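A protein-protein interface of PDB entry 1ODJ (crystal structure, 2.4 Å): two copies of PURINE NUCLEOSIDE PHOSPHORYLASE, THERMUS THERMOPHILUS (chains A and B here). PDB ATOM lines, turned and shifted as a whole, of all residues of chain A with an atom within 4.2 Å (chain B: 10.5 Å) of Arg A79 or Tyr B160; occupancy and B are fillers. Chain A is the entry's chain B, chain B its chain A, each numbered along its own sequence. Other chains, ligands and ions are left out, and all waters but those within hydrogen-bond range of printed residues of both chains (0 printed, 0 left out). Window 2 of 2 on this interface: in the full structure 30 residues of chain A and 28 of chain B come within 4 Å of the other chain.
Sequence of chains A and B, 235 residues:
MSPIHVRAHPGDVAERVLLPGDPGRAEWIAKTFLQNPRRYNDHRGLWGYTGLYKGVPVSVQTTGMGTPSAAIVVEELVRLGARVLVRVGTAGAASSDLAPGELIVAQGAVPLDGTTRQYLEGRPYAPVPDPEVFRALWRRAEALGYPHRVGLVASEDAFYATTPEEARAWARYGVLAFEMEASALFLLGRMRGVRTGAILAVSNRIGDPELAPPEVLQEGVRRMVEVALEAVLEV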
ATOM      1  N   ILE A   4     -12.960 -26.654  12.867  1.00  0.00           N
ATOM      2  CA  ILE A   4     -11.799 -27.336  13.410  1.00  0.00           C
ATOM      3  C   ILE A   4     -12.040 -28.727  14.002  1.00  0.00           C
ATOM      4  O   ILE A   4     -11.301 -29.670  13.709  1.00  0.00           O
ATOM      5  CB  ILE A   4     -11.130 -26.450  14.459  1.00  0.00           C
ATOM      6  CG1 ILE A   4     -10.549 -25.217  13.763  1.00  0.00           C
ATOM      7  CG2 ILE A   4     -10.056 -27.224  15.195  1.00  0.00           C
ATOM      8  CD1 ILE A   4      -9.746 -24.305  14.671  1.00  0.00           C
ATOM      9  N   GLU A  75     -20.755 -24.379  19.203  1.00  0.00           N
ATOM     10  CA  GLU A  75     -20.263 -23.254  18.411  1.00  0.00           C
ATOM     11  C   GLU A  75     -20.085 -23.670  16.957  1.00  0.00           C
ATOM     12  O   GLU A  75     -20.349 -22.894  16.041  1.00  0.00           O
ATOM     13  CB  GLU A  75     -18.916 -22.755  18.951  1.00  0.00           C
ATOM     14  CG  GLU A  75     -19.021 -21.882  20.197  1.00  0.00           C
ATOM     15  CD  GLU A  75     -19.418 -20.451  19.881  1.00  0.00           C
ATOM     16  OE1 GLU A  75     -20.041 -20.231  18.816  1.00  0.00           O
ATOM     17  OE2 GLU A  75     -19.116 -19.554  20.703  1.00  0.00           O
ATOM     18  N   GLU A  76     -19.654 -24.906  16.741  1.00  0.00           N
ATOM     19  CA  GLU A  76     -19.421 -25.358  15.385  1.00  0.00           C
ATOM     20  C   GLU A  76     -20.645 -25.898  14.661  1.00  0.00           C
ATOM     21  O   GLU A  76     -20.714 -25.833  13.433  1.00  0.00           O
ATOM     22  CB  GLU A  76     -18.264 -26.351  15.384  1.00  0.00           C
ATOM     23  CG  GLU A  76     -16.960 -25.669  15.814  1.00  0.00           C
ATOM     24  CD  GLU A  76     -15.730 -26.547  15.687  1.00  0.00           C
ATOM     25  OE1 GLU A  76     -15.773 -27.588  14.990  1.00  0.00           O
ATOM     26  OE2 GLU A  76     -14.700 -26.174  16.282  1.00  0.00           O
ATOM     27  N   LEU A  77     -21.619 -26.422  15.402  1.00  0.00           N
ATOM     28  CA  LEU A  77     -22.832 -26.907  14.753  1.00  0.00           C
ATOM     29  C   LEU A  77     -23.527 -25.676  14.174  1.00  0.00           C
ATOM     30  O   LEU A  77     -24.043 -25.708  13.063  1.00  0.00           O
ATOM     31  CB  LEU A  77     -23.767 -27.577  15.757  1.00  0.00           C
ATOM     32  CG  LEU A  77     -23.513 -29.011  16.214  1.00  0.00           C
ATOM     33  CD1 LEU A  77     -24.294 -29.240  17.485  1.00  0.00           C
ATOM     34  CD2 LEU A  77     -23.919 -30.006  15.141  1.00  0.00           C
ATOM     35  N   VAL A  78     -23.509 -24.588  14.939  1.00  0.00           N
ATOM     36  CA  VAL A  78     -24.142 -23.340  14.533  1.00  0.00           C
ATOM     37  C   VAL A  78     -23.602 -22.785  13.216  1.00  0.00           C
ATOM     38  O   VAL A  78     -24.382 -22.430  12.340  1.00  0.00           O
ATOM     39  CB  VAL A  78     -23.995 -22.265  15.634  1.00  0.00           C
ATOM     40  CG1 VAL A  78     -24.789 -21.008  15.265  1.00  0.00           C
ATOM     41  CG2 VAL A  78     -24.466 -22.824  16.965  1.00  0.00           C
ATOM     42  N   ARG A  79     -22.277 -22.700  13.077  1.00  0.00           N
ATOM     43  CA  ARG A  79     -21.678 -22.195  11.840  1.00  0.00           C
ATOM     44  C   ARG A  79     -21.888 -23.226  10.741  1.00  0.00           C
ATOM     45  O   ARG A  79     -21.561 -22.981   9.581  1.00  0.00           O
ATOM     46  CB  ARG A  79     -20.167 -21.968  11.982  1.00  0.00           C
ATOM     47  CG  ARG A  79     -19.705 -21.045  13.102  1.00  0.00           C
ATOM     48  CD  ARG A  79     -18.189 -20.825  12.991  1.00  0.00           C
ATOM     49  NE  ARG A  79     -17.531 -20.578  14.276  1.00  0.00           N
ATOM     50  CZ  ARG A  79     -17.764 -19.522  15.049  1.00  0.00           C
ATOM     51  NH1 ARG A  79     -18.644 -18.602  14.674  1.00  0.00           N
ATOM     52  NH2 ARG A  79     -17.115 -19.383  16.198  1.00  0.00           N
ATOM     53  N   LEU A  80     -22.420 -24.385  11.118  1.00  0.00           N
ATOM     54  CA  LEU A  80     -22.670 -25.472  10.176  1.00  0.00           C
ATOM     55  C   LEU A  80     -24.139 -25.613   9.776  1.00  0.00           C
ATOM     56  O   LEU A  80     -24.479 -26.440   8.931  1.00  0.00           O
ATOM     57  CB  LEU A  80     -22.180 -26.802  10.760  1.00  0.00           C
ATOM     58  CG  LEU A  80     -20.682 -27.090  10.695  1.00  0.00           C
ATOM     59  CD1 LEU A  80     -20.377 -28.436  11.381  1.00  0.00           C
ATOM     60  CD2 LEU A  80     -20.248 -27.116   9.233  1.00  0.00           C
ATOM     61  N   GLY A  81     -25.006 -24.816  10.390  1.00  0.00           N
ATOM     62  CA  GLY A  81     -26.416 -24.881  10.057  1.00  0.00           C
ATOM     63  C   GLY A  81     -27.367 -25.184  11.197  1.00  0.00           C
ATOM     64  O   GLY A  81     -28.572 -24.976  11.059  1.00  0.00           O
ATOM     65  N   TYR A 119     -17.189 -17.213  29.233  1.00  0.00           N
ATOM     66  CA  TYR A 119     -18.004 -16.512  28.237  1.00  0.00           C
ATOM     67  C   TYR A 119     -18.706 -15.273  28.807  1.00  0.00           C
ATOM     68  O   TYR A 119     -18.887 -14.277  28.105  1.00  0.00           O
ATOM     69  CB  TYR A 119     -19.074 -17.443  27.658  1.00  0.00           C
ATOM     70  CG  TYR A 119     -18.665 -18.246  26.438  1.00  0.00           C
ATOM     71  CD1 TYR A 119     -18.482 -19.628  26.521  1.00  0.00           C
ATOM     72  CD2 TYR A 119     -18.561 -17.644  25.186  1.00  0.00           C
ATOM     73  CE1 TYR A 119     -18.220 -20.391  25.396  1.00  0.00           C
ATOM     74  CE2 TYR A 119     -18.303 -18.405  24.042  1.00  0.00           C
ATOM     75  CZ  TYR A 119     -18.136 -19.782  24.159  1.00  0.00           C
ATOM     76  OH  TYR A 119     -17.904 -20.551  23.037  1.00  0.00           O
ATOM     77  N   MET B  65     -11.616 -33.464  25.412  1.00  0.00           N
ATOM     78  CA  MET B  65     -11.284 -32.043  25.441  1.00  0.00           C
ATOM     79  C   MET B  65     -11.859 -31.369  26.682  1.00  0.00           C
ATOM     80  O   MET B  65     -13.051 -31.493  26.973  1.00  0.00           O
ATOM     81  CB  MET B  65     -11.799 -31.339  24.180  1.00  0.00           C
ATOM     82  CG  MET B  65     -11.143 -31.809  22.885  1.00  0.00           C
ATOM     83  SD  MET B  65     -11.541 -30.767  21.458  1.00  0.00           S
ATOM     84  CE  MET B  65     -13.171 -31.374  21.091  1.00  0.00           C
ATOM     85  N   GLU B 156      -7.671 -23.132  29.575  1.00  0.00           N
ATOM     86  CA  GLU B 156      -8.972 -22.484  29.587  1.00  0.00           C
ATOM     87  C   GLU B 156     -10.114 -23.475  29.350  1.00  0.00           C
ATOM     88  O   GLU B 156      -9.883 -24.653  29.078  1.00  0.00           O
ATOM     89  CB  GLU B 156      -9.028 -21.342  28.560  1.00  0.00           C
ATOM     90  CG  GLU B 156      -8.722 -21.736  27.124  1.00  0.00           C
ATOM     91  CD  GLU B 156      -8.821 -20.549  26.169  1.00  0.00           C
ATOM     92  OE1 GLU B 156      -8.565 -20.734  24.962  1.00  0.00           O
ATOM     93  OE2 GLU B 156      -9.158 -19.429  26.616  1.00  0.00           O
ATOM     94  N   ASP B 157     -11.343 -22.979  29.467  1.00  0.00           N
ATOM     95  CA  ASP B 157     -12.552 -23.778  29.288  1.00  0.00           C
ATOM     96  C   ASP B 157     -13.246 -23.509  27.960  1.00  0.00           C
ATOM     97  O   ASP B 157     -13.696 -24.429  27.290  1.00  0.00           O
ATOM     98  CB  ASP B 157     -13.538 -23.482  30.419  1.00  0.00           C
ATOM     99  CG  ASP B 157     -13.231 -24.265  31.673  1.00  0.00           C
ATOM    100  OD1 ASP B 157     -13.724 -23.875  32.754  1.00  0.00           O
ATOM    101  OD2 ASP B 157     -12.510 -25.282  31.580  1.00  0.00           O
ATOM    102  N   ALA B 158     -13.332 -22.235  27.601  1.00  0.00           N
ATOM    103  CA  ALA B 158     -13.999 -21.813  26.383  1.00  0.00           C
ATOM    104  C   ALA B 158     -13.023 -21.547  25.260  1.00  0.00           C
ATOM    105  O   ALA B 158     -12.445 -20.465  25.178  1.00  0.00           O
ATOM    106  CB  ALA B 158     -14.817 -20.565  26.659  1.00  0.00           C
ATOM    107  N   PHE B 159     -12.863 -22.542  24.391  1.00  0.00           N
ATOM    108  CA  PHE B 159     -11.968 -22.476  23.241  1.00  0.00           C
ATOM    109  C   PHE B 159     -12.214 -21.213  22.419  1.00  0.00           C
ATOM    110  O   PHE B 159     -11.281 -20.449  22.145  1.00  0.00           O
ATOM    111  CB  PHE B 159     -12.202 -23.706  22.365  1.00  0.00           C
ATOM    112  CG  PHE B 159     -11.229 -23.855  21.240  1.00  0.00           C
ATOM    113  CD1 PHE B 159     -10.002 -24.482  21.438  1.00  0.00           C
ATOM    114  CD2 PHE B 159     -11.544 -23.399  19.970  1.00  0.00           C
ATOM    115  CE1 PHE B 159      -9.097 -24.659  20.376  1.00  0.00           C
ATOM    116  CE2 PHE B 159     -10.648 -23.570  18.903  1.00  0.00           C
ATOM    117  CZ  PHE B 159      -9.421 -24.205  19.112  1.00  0.00           C
ATOM    118  N   TYR B 160     -13.476 -21.008  22.034  1.00  0.00           N
ATOM    119  CA  TYR B 160     -13.895 -19.865  21.223  1.00  0.00           C
ATOM    120  C   TYR B 160     -14.233 -18.574  21.960  1.00  0.00           C
ATOM    121  O   TYR B 160     -14.989 -17.750  21.450  1.00  0.00           O
ATOM    122  CB  TYR B 160     -15.099 -20.237  20.362  1.00  0.00           C
ATOM    123  CG  TYR B 160     -14.795 -21.197  19.241  1.00  0.00           C
ATOM    124  CD1 TYR B 160     -15.117 -22.543  19.348  1.00  0.00           C
ATOM    125  CD2 TYR B 160     -14.171 -20.758  18.074  1.00  0.00           C
ATOM    126  CE1 TYR B 160     -14.826 -23.437  18.321  1.00  0.00           C
ATOM    127  CE2 TYR B 160     -13.870 -21.642  17.041  1.00  0.00           C
ATOM    128  CZ  TYR B 160     -14.198 -22.981  17.173  1.00  0.00           C
ATOM    129  OH  TYR B 160     -13.872 -23.864  16.171  1.00  0.00           O
ATOM    130  N   ALA B 161     -13.696 -18.382  23.155  1.00  0.00           N
ATOM    131  CA  ALA B 161     -13.952 -17.151  23.892  1.00  0.00           C
ATOM    132  C   ALA B 161     -12.754 -16.215  23.787  1.00  0.00           C
ATOM    133  O   ALA B 161     -12.913 -15.008  23.608  1.00  0.00           O
ATOM    134  CB  ALA B 161     -14.239 -17.461  25.346  1.00  0.00           C
ATOM    135  N   THR B 162     -11.555 -16.777  23.886  1.00  0.00           N
ATOM    136  CA  THR B 162     -10.329 -15.994  23.822  1.00  0.00           C
ATOM    137  C   THR B 162     -10.108 -15.457  22.419  1.00  0.00           C
ATOM    138  O   THR B 162     -10.375 -16.146  21.445  1.00  0.00           O
ATOM    139  CB  THR B 162      -9.114 -16.860  24.251  1.00  0.00           C
ATOM    140  OG1 THR B 162      -9.292 -17.280  25.612  1.00  0.00           O
ATOM    141  CG2 THR B 162      -7.808 -16.081  24.139  1.00  0.00           C
ATOM    142  N   THR B 163      -9.630 -14.221  22.325  1.00  0.00           N
ATOM    143  CA  THR B 163      -9.352 -13.587  21.035  1.00  0.00           C
ATOM    144  C   THR B 163      -7.844 -13.368  20.898  1.00  0.00           C
ATOM    145  O   THR B 163      -7.103 -13.424  21.880  1.00  0.00           O
ATOM    146  CB  THR B 163     -10.029 -12.205  20.912  1.00  0.00           C
ATOM    147  OG1 THR B 163      -9.268 -11.236  21.644  1.00  0.00           O
ATOM    148  CG2 THR B 163     -11.437 -12.247  21.475  1.00  0.00           C
ATOM    149  N   PRO B 164      -7.366 -13.096  19.677  1.00  0.00           N
ATOM    150  CA  PRO B 164      -5.924 -12.880  19.508  1.00  0.00           C
ATOM    151  C   PRO B 164      -5.379 -11.815  20.465  1.00  0.00           C
ATOM    152  O   PRO B 164      -4.208 -11.841  20.831  1.00  0.00           O
ATOM    153  CB  PRO B 164      -5.807 -12.448  18.046  1.00  0.00           C
ATOM    154  CG  PRO B 164      -6.973 -13.147  17.391  1.00  0.00           C
ATOM    155  CD  PRO B 164      -8.082 -12.950  18.396  1.00  0.00           C
ATOM    156  N   GLU B 166      -6.664 -10.911  23.765  1.00  0.00           N
ATOM    157  CA  GLU B 166      -6.622 -11.360  25.153  1.00  0.00           C
ATOM    158  C   GLU B 166      -5.527 -12.386  25.378  1.00  0.00           C
ATOM    159  O   GLU B 166      -4.929 -12.434  26.450  1.00  0.00           O
ATOM    160  CB  GLU B 166      -7.959 -11.977  25.537  1.00  0.00           C
ATOM    161  CG  GLU B 166      -9.156 -11.313  24.890  1.00  0.00           C
ATOM    162  CD  GLU B 166     -10.455 -11.885  25.397  1.00  0.00           C
ATOM    163  OE1 GLU B 166     -10.557 -13.132  25.472  1.00  0.00           O
ATOM    164  OE2 GLU B 166     -11.367 -11.094  25.720  1.00  0.00           O
ATOM    165  N   PHE B 178      -2.018 -21.737  24.789  1.00  0.00           N
ATOM    166  CA  PHE B 178      -3.271 -22.147  25.398  1.00  0.00           C
ATOM    167  C   PHE B 178      -3.646 -23.584  25.061  1.00  0.00           C
ATOM    168  O   PHE B 178      -3.418 -24.050  23.938  1.00  0.00           O
ATOM    169  CB  PHE B 178      -4.408 -21.191  24.977  1.00  0.00           C
ATOM    170  CG  PHE B 178      -4.329 -19.818  25.613  1.00  0.00           C
ATOM    171  CD1 PHE B 178      -3.300 -18.928  25.283  1.00  0.00           C
ATOM    172  CD2 PHE B 178      -5.276 -19.416  26.543  1.00  0.00           C
ATOM    173  CE1 PHE B 178      -3.217 -17.656  25.876  1.00  0.00           C
ATOM    174  CE2 PHE B 178      -5.198 -18.144  27.141  1.00  0.00           C
ATOM    175  CZ  PHE B 178      -4.163 -17.269  26.801  1.00  0.00           C
ATOM    176  N   GLU B 179      -4.201 -24.274  26.060  1.00  0.00           N
ATOM    177  CA  GLU B 179      -4.655 -25.655  25.930  1.00  0.00           C
ATOM    178  C   GLU B 179      -5.830 -25.902  26.888  1.00  0.00           C
ATOM    179  O   GLU B 179      -6.304 -24.972  27.532  1.00  0.00           O
ATOM    180  CB  GLU B 179      -3.492 -26.647  26.158  1.00  0.00           C
ATOM    181  CG  GLU B 179      -2.656 -26.464  27.419  1.00  0.00           C
ATOM    182  CD  GLU B 179      -3.118 -27.339  28.567  1.00  0.00           C
ATOM    183  OE1 GLU B 179      -3.782 -26.808  29.483  1.00  0.00           O
ATOM    184  OE2 GLU B 179      -2.822 -28.558  28.551  1.00  0.00           O
ATOM    185  N   MET B 180      -6.307 -27.137  26.989  1.00  0.00           N
ATOM    186  CA  MET B 180      -7.469 -27.398  27.838  1.00  0.00           C
ATOM    187  C   MET B 180      -7.440 -28.612  28.762  1.00  0.00           C
ATOM    188  O   MET B 180      -8.468 -29.257  28.945  1.00  0.00           O
ATOM    189  CB  MET B 180      -8.733 -27.476  26.956  1.00  0.00           C
ATOM    190  CG  MET B 180      -9.185 -26.122  26.389  1.00  0.00           C
ATOM    191  SD  MET B 180     -10.392 -26.181  25.003  1.00  0.00           S
ATOM    192  CE  MET B 180     -11.814 -27.029  25.813  1.00  0.00           C
ATOM    193  N   ASN B 204      -0.821 -24.107  16.127  1.00  0.00           N
ATOM    194  CA  ASN B 204      -1.173 -22.859  15.450  1.00  0.00           C
ATOM    195  C   ASN B 204      -1.019 -21.639  16.362  1.00  0.00           C
ATOM    196  O   ASN B 204      -0.861 -21.763  17.577  1.00  0.00           O
ATOM    197  CB  ASN B 204      -2.621 -22.912  14.961  1.00  0.00           C
ATOM    198  CG  ASN B 204      -3.605 -23.083  16.099  1.00  0.00           C
ATOM    199  OD1 ASN B 204      -4.079 -24.187  16.364  1.00  0.00           O
ATOM    200  ND2 ASN B 204      -3.904 -21.988  16.796  1.00  0.00           N
ATOM    201  N   ILE B 206      -2.714 -18.270  17.912  1.00  0.00           N
ATOM    202  CA  ILE B 206      -4.055 -17.781  18.214  1.00  0.00           C
ATOM    203  C   ILE B 206      -4.504 -16.679  17.251  1.00  0.00           C
ATOM    204  O   ILE B 206      -3.849 -15.638  17.127  1.00  0.00           O
ATOM    205  CB  ILE B 206      -4.127 -17.252  19.660  1.00  0.00           C
ATOM    206  CG1 ILE B 206      -3.903 -18.403  20.642  1.00  0.00           C
ATOM    207  CG2 ILE B 206      -5.469 -16.588  19.913  1.00  0.00           C
ATOM    208  CD1 ILE B 206      -4.959 -19.476  20.581  1.00  0.00           C
ATOM    209  N   GLY B 207      -5.624 -16.925  16.572  1.00  0.00           N
ATOM    210  CA  GLY B 207      -6.161 -15.965  15.622  1.00  0.00           C
ATOM    211  C   GLY B 207      -6.425 -16.538  14.235  1.00  0.00           C
ATOM    212  O   GLY B 207      -7.005 -15.869  13.372  1.00  0.00           O
ATOM    213  N   ASP B 208      -6.000 -17.781  14.023  1.00  0.00           N
ATOM    214  CA  ASP B 208      -6.170 -18.460  12.740  1.00  0.00           C
ATOM    215  C   ASP B 208      -7.357 -19.423  12.709  1.00  0.00           C
ATOM    216  O   ASP B 208      -7.572 -20.195  13.650  1.00  0.00           O
ATOM    217  CB  ASP B 208      -4.883 -19.202  12.384  1.00  0.00           C
ATOM    218  CG  ASP B 208      -3.759 -18.259  12.026  1.00  0.00           C
ATOM    219  OD1 ASP B 208      -3.838 -17.634  10.943  1.00  0.00           O
ATOM    220  OD2 ASP B 208      -2.805 -18.131  12.825  1.00  0.00           O
ATOM    221  N   PRO B 209      -8.138 -19.392  11.614  1.00  0.00           N
ATOM    222  CA  PRO B 209      -9.326 -20.232  11.396  1.00  0.00           C
ATOM    223  C   PRO B 209      -9.123 -21.755  11.464  1.00  0.00           C
ATOM    224  O   PRO B 209     -10.092 -22.504  11.624  1.00  0.00           O
ATOM    225  CB  PRO B 209      -9.816 -19.775  10.020  1.00  0.00           C
ATOM    226  CG  PRO B 209      -9.409 -18.335   9.988  1.00  0.00           C
ATOM    227  CD  PRO B 209      -8.002 -18.404  10.530  1.00  0.00           C
ATOM    228  N   GLU B 210      -7.878 -22.210  11.340  1.00  0.00           N
ATOM    229  CA  GLU B 210      -7.577 -23.642  11.390  1.00  0.00           C
ATOM    230  C   GLU B 210      -6.178 -23.896  11.972  1.00  0.00           C
ATOM    231  O   GLU B 210      -5.878 -23.457  13.088  1.00  0.00           O
ATOM    232  CB  GLU B 210      -7.690 -24.255   9.984  1.00  0.00           C
ATOM    233  CG  GLU B 210      -9.079 -24.127   9.345  1.00  0.00           C
ATOM    234  CD  GLU B 210      -9.102 -24.548   7.878  1.00  0.00           C
ATOM    235  OE1 GLU B 210     -10.146 -24.347   7.219  1.00  0.00           O
ATOM    236  OE2 GLU B 210      -8.079 -25.078   7.392  1.00  0.00           O
ATOM    237  N   LEU B 211      -5.327 -24.599  11.219  1.00  0.00           N
ATOM    238  CA  LEU B 211      -3.964 -24.909  11.668  1.00  0.00           C
ATOM    239  C   LEU B 211      -2.894 -24.606  10.586  1.00  0.00           C
ATOM    240  O   LEU B 211      -3.180 -23.942   9.584  1.00  0.00           O
ATOM    241  CB  LEU B 211      -3.888 -26.379  12.125  1.00  0.00           C
ATOM    242  CG  LEU B 211      -5.022 -26.932  13.017  1.00  0.00           C
ATOM    243  CD1 LEU B 211      -4.664 -28.343  13.487  1.00  0.00           C
ATOM    244  CD2 LEU B 211      -5.258 -26.030  14.224  1.00  0.00           C
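The side-chain hydroxyl of Tyr B160 sits at hydrogen-bond distance from the side-chain carboxylate of Glu A76, 2.5 Å away.
The side-chain carboxylate (OE2) of Glu A75 lies within hydrogen-bond range of the side-chain hydroxyl (OH) of Tyr A119 (2.8 Å).
Pro B209 touches Ile A4. Ile A4 touches Glu B210 (CD1 to CA, 3.99 Å). Tyr B160 touches Glu A75. NH2 of Arg A79 touches CD2 of Tyr B160 (3.8 Å). CB of Ala B158 touches CE1 of Tyr A119, 3.6 Å away. Tyr B160 touches Tyr A119.
Of the printed residues of chain B, Ile A4 touches Pro B209 (3.5 Å) and Glu B210 (3.99 Å). No residue of chain B comes within 4 Å of Val A78. Printed residues of chain B within 4 Å of Tyr A119: Ala B158 and Tyr B160. Of the printed residues of chain A, Ala B158 touches Tyr A119 (3.6 Å). Of the printed residues of chain A, Pro B209 touches Ile A4. Of the printed residues of chain A, Glu B210 touches Ile A4. The nearest residue of chain A that does not touch Tyr B160 is Ile A4 (4.1 Å). The nearest printed residue of chain A that does not touch Glu B210 is Glu A76 (9.0 Å).
Of the 9 printed residues of chain A, 5 touch a printed residue of chain B. Printed residues of chain B that touch a printed residue of chain A: Ala B158, Tyr B160, Pro B209 and Glu B210. Hydrophobic or aromatic side chains of chain B within 4 Å of the printed part of chain A: Ala B158 and Tyr B160. Among the printed residues, 7 pairs touch across the chains. Among the printed residues, no Asp or Glu carboxylate lies within 4 Å of a Lys or Arg side-chain nitrogen of the other chain.
No position is printed for both chains. Of the 7 pairs that touch across the chains among the printed residues, none has its exchanged pair printed and touching as well.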
